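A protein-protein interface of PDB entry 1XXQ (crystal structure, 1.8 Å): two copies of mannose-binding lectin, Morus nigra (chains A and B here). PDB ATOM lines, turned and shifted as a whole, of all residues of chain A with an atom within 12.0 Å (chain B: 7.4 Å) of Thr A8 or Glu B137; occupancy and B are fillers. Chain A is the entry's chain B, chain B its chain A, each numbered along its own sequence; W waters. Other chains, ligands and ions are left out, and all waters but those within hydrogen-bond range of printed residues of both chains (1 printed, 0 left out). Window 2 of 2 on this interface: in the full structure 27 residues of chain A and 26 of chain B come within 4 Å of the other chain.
Along chain B the printed residues that touch a printed residue of chain A span positions 88 to 139.
Along chain A the printed residues that touch a printed residue of chain B span positions 8 to 12.
Among the printed residues, 9 pairs touch across the chains.
Among the printed residues, no Asp or Glu carboxylate lies within 4 Å of a Lys or Arg side-chain nitrogen of the other chain.
Thr A8 touches Glu B137.
Phe B88 touches Gln A9 (CZ to O, 3.4 Å).
Asn B138 touches Gln A9.
Thr A10 touches Phe B88 (C to CE2, 3.6 Å).
C of Thr A11 touches CD2 of Phe B88 (3.5 Å).
N of Gly A12 touches CD2 of Phe B88, at 3.5 Å.
Water W1 lies within hydrogen-bond range of the side-chain amide nitrogen (ND2) of Asn B138 (2.9 Å) and the backbone carbonyl oxygen (O) of Thr A8 (3.4 Å).
N of Gly B139 sits close to NE2 of Gln A9, 2.8 Å away.
The backbone NH (N) of Gln A9 sits at hydrogen-bond distance from the backbone carbonyl oxygen (O) of Glu B137 (3.4 Å).
The backbone NH (N) of Thr A8 lies close to the side-chain amide nitrogen (ND2) of Asn B138, 3.1 Å away.
No position is printed for both chains.
Of the 9 pairs that touch across the chains among the printed residues, none has its exchanged pair printed and touching as well.
Of chain B, only Glu B137 (3.2 Å) and Asn B138 (3.1 Å) come within 4 Å of Thr A8.
Glu B137 touches just these residues of chain A: Thr A8 (3.2 Å) and Gln A9 (3.4 Å).
Pro B135 touches none of the printed residues of chain A.
No residue of chain A comes within 4 Å of Ile B136.
Asn B138 touches just these residues of chain A: Thr A8 (3.1 Å) and Gln A9 (3.6 Å).
Gly B139 touches just one residue of chain A: Gln A9 (2.8 Å).
Of the printed residues of chain B, Gln A9 touches Phe B88 (3.4 Å), Glu B137 (3.4 Å), Asn B138 (3.6 Å) and Gly B139 (2.8 Å).
Of the printed residues of chain B, Thr A10 touches Phe B88 (3.6 Å).
Printed residues of chain B within 4 Å of Thr A11: Phe B88 (3.5 Å).
Of the printed residues of chain B, Gly A12 touches Phe B88 (3.5 Å).
Printed residues of chain A within 4 Å of Phe B88: Gln A9, Thr A10, Thr A11 and Gly A12.
Gln A15 touches none of the printed residues of chain B.
The nearest residue of chain B that does not touch Thr A8 is Gly B139 (5.5 Å).
The backbone carbonyl oxygen (O) of Thr A11 lies close to the side-chain amide oxygen (OE1) of Gln A9 (2.8 Å).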
ATOM      1  N   THR A   8      15.839  21.762 -13.973  1.00  0.00           N
ATOM      2  CA  THR A   8      16.560  21.920 -12.680  1.00  0.00           C
ATOM      3  C   THR A   8      17.897  21.196 -12.737  1.00  0.00           C
ATOM      4  O   THR A   8      17.982  20.070 -13.229  1.00  0.00           O
ATOM      5  CB  THR A   8      15.736  21.347 -11.513  1.00  0.00           C
ATOM      6  OG1 THR A   8      14.464  22.004 -11.460  1.00  0.00           O
ATOM      7  CG2 THR A   8      16.464  21.556 -10.192  1.00  0.00           C
ATOM      8  N   GLN A   9      18.943  21.842 -12.236  1.00  0.00           N
ATOM      9  CA  GLN A   9      20.268  21.242 -12.252  1.00  0.00           C
ATOM     10  C   GLN A   9      20.424  20.275 -11.083  1.00  0.00           C
ATOM     11  O   GLN A   9      20.149  20.626  -9.936  1.00  0.00           O
ATOM     12  CB  GLN A   9      21.343  22.331 -12.179  1.00  0.00           C
ATOM     13  CG  GLN A   9      22.725  21.828 -12.541  1.00  0.00           C
ATOM     14  CD  GLN A   9      22.791  21.283 -13.955  1.00  0.00           C
ATOM     15  OE1 GLN A   9      23.585  20.385 -14.249  1.00  0.00           O
ATOM     16  NE2 GLN A   9      21.967  21.832 -14.845  1.00  0.00           N
ATOM     17  N   THR A  10      20.872  19.059 -11.374  1.00  0.00           N
ATOM     18  CA  THR A  10      21.040  18.056 -10.329  1.00  0.00           C
ATOM     19  C   THR A  10      22.445  17.467 -10.262  1.00  0.00           C
ATOM     20  O   THR A  10      22.744  16.669  -9.375  1.00  0.00           O
ATOM     21  CB  THR A  10      20.031  16.904 -10.501  1.00  0.00           C
ATOM     22  OG1 THR A  10      20.194  16.310 -11.795  1.00  0.00           O
ATOM     23  CG2 THR A  10      18.608  17.421 -10.363  1.00  0.00           C
ATOM     24  N   THR A  11      23.305  17.857 -11.197  1.00  0.00           N
ATOM     25  CA  THR A  11      24.678  17.363 -11.212  1.00  0.00           C
ATOM     26  C   THR A  11      25.642  18.495 -11.552  1.00  0.00           C
ATOM     27  O   THR A  11      25.258  19.471 -12.193  1.00  0.00           O
ATOM     28  CB  THR A  11      24.861  16.234 -12.240  1.00  0.00           C
ATOM     29  OG1 THR A  11      26.184  15.700 -12.123  1.00  0.00           O
ATOM     30  CG2 THR A  11      24.655  16.756 -13.654  1.00  0.00           C
ATOM     31  N   GLY A  12      26.895  18.356 -11.127  1.00  0.00           N
ATOM     32  CA  GLY A  12      27.884  19.385 -11.388  1.00  0.00           C
ATOM     33  C   GLY A  12      28.654  19.230 -12.686  1.00  0.00           C
ATOM     34  O   GLY A  12      29.493  20.072 -13.012  1.00  0.00           O
ATOM     35  N   THR A  13      28.383  18.162 -13.429  1.00  0.00           N
ATOM     36  CA  THR A  13      29.073  17.927 -14.691  1.00  0.00           C
ATOM     37  C   THR A  13      28.200  18.349 -15.867  1.00  0.00           C
ATOM     38  O   THR A  13      27.042  17.936 -15.969  1.00  0.00           O
ATOM     39  CB  THR A  13      29.444  16.441 -14.858  1.00  0.00           C
ATOM     40  OG1 THR A  13      30.247  16.021 -13.747  1.00  0.00           O
ATOM     41  CG2 THR A  13      30.233  16.231 -16.146  1.00  0.00           C
ATOM     42  N   SER A  14      28.756  19.174 -16.746  1.00  0.00           N
ATOM     43  CA  SER A  14      28.018  19.642 -17.916  1.00  0.00           C
ATOM     44  C   SER A  14      27.834  18.488 -18.897  1.00  0.00           C
ATOM     45  O   SER A  14      28.422  17.416 -18.733  1.00  0.00           O
ATOM     46  CB  SER A  14      28.763  20.802 -18.591  1.00  0.00           C
ATOM     47  OG  SER A  14      30.015  20.384 -19.105  1.00  0.00           O
ATOM     48  N   GLN A  15      27.023  18.699 -19.925  1.00  0.00           N
ATOM     49  CA  GLN A  15      26.787  17.631 -20.884  1.00  0.00           C
ATOM     50  C   GLN A  15      26.666  18.136 -22.308  1.00  0.00           C
ATOM     51  O   GLN A  15      26.551  19.337 -22.554  1.00  0.00           O
ATOM     52  CB  GLN A  15      25.512  16.871 -20.510  1.00  0.00           C
ATOM     53  CG  GLN A  15      24.253  17.717 -20.591  1.00  0.00           C
ATOM     54  CD  GLN A  15      23.054  17.059 -19.925  1.00  0.00           C
ATOM     55  OE1 GLN A  15      22.324  17.703 -19.165  1.00  0.00           O
ATOM     56  NE2 GLN A  15      22.836  15.778 -20.214  1.00  0.00           N
ATOM     57  N   PHE B  88      27.612  22.022  -6.668  1.00  0.00           N
ATOM     58  CA  PHE B  88      27.829  22.936  -7.781  1.00  0.00           C
ATOM     59  C   PHE B  88      27.110  24.255  -7.536  1.00  0.00           C
ATOM     60  O   PHE B  88      26.120  24.313  -6.807  1.00  0.00           O
ATOM     61  CB  PHE B  88      27.337  22.289  -9.081  1.00  0.00           C
ATOM     62  CG  PHE B  88      25.935  21.757  -8.993  1.00  0.00           C
ATOM     63  CD1 PHE B  88      24.845  22.589  -9.223  1.00  0.00           C
ATOM     64  CD2 PHE B  88      25.706  20.435  -8.623  1.00  0.00           C
ATOM     65  CE1 PHE B  88      23.547  22.116  -9.084  1.00  0.00           C
ATOM     66  CE2 PHE B  88      24.407  19.950  -8.481  1.00  0.00           C
ATOM     67  CZ  PHE B  88      23.327  20.793  -8.711  1.00  0.00           C
ATOM     68  N   VAL B  90      24.745  27.348  -7.745  1.00  0.00           N
ATOM     69  CA  VAL B  90      23.366  27.575  -8.159  1.00  0.00           C
ATOM     70  C   VAL B  90      23.136  29.083  -8.213  1.00  0.00           C
ATOM     71  O   VAL B  90      22.064  29.554  -8.596  1.00  0.00           O
ATOM     72  CB  VAL B  90      22.353  26.919  -7.186  1.00  0.00           C
ATOM     73  CG1 VAL B  90      22.586  25.410  -7.141  1.00  0.00           C
ATOM     74  CG2 VAL B  90      22.476  27.521  -5.799  1.00  0.00           C
ATOM     75  N   SER B  91      24.161  29.837  -7.829  1.00  0.00           N
ATOM     76  CA  SER B  91      24.084  31.293  -7.854  1.00  0.00           C
ATOM     77  C   SER B  91      25.402  31.966  -7.510  1.00  0.00           C
ATOM     78  O   SER B  91      26.153  31.493  -6.661  1.00  0.00           O
ATOM     79  CB  SER B  91      23.016  31.795  -6.875  1.00  0.00           C
ATOM     80  OG  SER B  91      23.046  33.211  -6.776  1.00  0.00           O
ATOM     81  N   LEU B 134      23.375  36.348 -10.224  1.00  0.00           N
ATOM     82  CA  LEU B 134      23.017  35.433 -11.286  1.00  0.00           C
ATOM     83  C   LEU B 134      22.521  34.125 -10.702  1.00  0.00           C
ATOM     84  O   LEU B 134      23.294  33.184 -10.518  1.00  0.00           O
ATOM     85  CB  LEU B 134      24.205  35.146 -12.209  1.00  0.00           C
ATOM     86  CG  LEU B 134      23.835  34.179 -13.343  1.00  0.00           C
ATOM     87  CD1 LEU B 134      22.942  34.899 -14.353  1.00  0.00           C
ATOM     88  CD2 LEU B 134      25.080  33.651 -14.018  1.00  0.00           C
ATOM     89  N   PRO B 135      21.233  34.063 -10.349  1.00  0.00           N
ATOM     90  CA  PRO B 135      20.714  32.812  -9.802  1.00  0.00           C
ATOM     91  C   PRO B 135      20.514  31.896 -11.005  1.00  0.00           C
ATOM     92  O   PRO B 135      20.120  32.356 -12.078  1.00  0.00           O
ATOM     93  CB  PRO B 135      19.401  33.236  -9.147  1.00  0.00           C
ATOM     94  CG  PRO B 135      18.976  34.416  -9.950  1.00  0.00           C
ATOM     95  CD  PRO B 135      20.259  35.158 -10.200  1.00  0.00           C
ATOM     96  N   ILE B 136      20.808  30.612 -10.841  1.00  0.00           N
ATOM     97  CA  ILE B 136      20.669  29.661 -11.938  1.00  0.00           C
ATOM     98  C   ILE B 136      19.670  28.574 -11.571  1.00  0.00           C
ATOM     99  O   ILE B 136      19.771  27.970 -10.503  1.00  0.00           O
ATOM    100  CB  ILE B 136      22.028  29.001 -12.267  1.00  0.00           C
ATOM    101  CG1 ILE B 136      23.051  30.082 -12.632  1.00  0.00           C
ATOM    102  CG2 ILE B 136      21.864  28.001 -13.414  1.00  0.00           C
ATOM    103  CD1 ILE B 136      24.475  29.572 -12.728  1.00  0.00           C
ATOM    104  N   GLU B 137      18.703  28.336 -12.455  1.00  0.00           N
ATOM    105  CA  GLU B 137      17.689  27.311 -12.225  1.00  0.00           C
ATOM    106  C   GLU B 137      17.983  26.030 -12.998  1.00  0.00           C
ATOM    107  O   GLU B 137      17.638  24.938 -12.552  1.00  0.00           O
ATOM    108  CB  GLU B 137      16.302  27.822 -12.620  1.00  0.00           C
ATOM    109  CG  GLU B 137      15.693  28.814 -11.644  1.00  0.00           C
ATOM    110  CD  GLU B 137      14.267  29.180 -12.018  1.00  0.00           C
ATOM    111  OE1 GLU B 137      13.651  29.996 -11.303  1.00  0.00           O
ATOM    112  OE2 GLU B 137      13.765  28.646 -13.030  1.00  0.00           O
ATOM    113  N   ASN B 138      18.609  26.167 -14.161  1.00  0.00           N
ATOM    114  CA  ASN B 138      18.950  25.008 -14.983  1.00  0.00           C
ATOM    115  C   ASN B 138      20.232  25.334 -15.731  1.00  0.00           C
ATOM    116  O   ASN B 138      20.328  26.371 -16.387  1.00  0.00           O
ATOM    117  CB  ASN B 138      17.831  24.708 -15.990  1.00  0.00           C
ATOM    118  CG  ASN B 138      17.919  23.298 -16.564  1.00  0.00           C
ATOM    119  OD1 ASN B 138      17.639  23.075 -17.745  1.00  0.00           O
ATOM    120  ND2 ASN B 138      18.291  22.340 -15.725  1.00  0.00           N
ATOM    121  N   GLY B 139      21.218  24.452 -15.633  1.00  0.00           N
ATOM    122  CA  GLY B 139      22.480  24.700 -16.303  1.00  0.00           C
ATOM    123  C   GLY B 139      23.599  24.911 -15.300  1.00  0.00           C
ATOM    124  O   GLY B 139      23.364  24.939 -14.087  1.00  0.00           O
HETATM  125  O   HOH W   1      19.392  19.702 -16.273  1.00  0.00           O
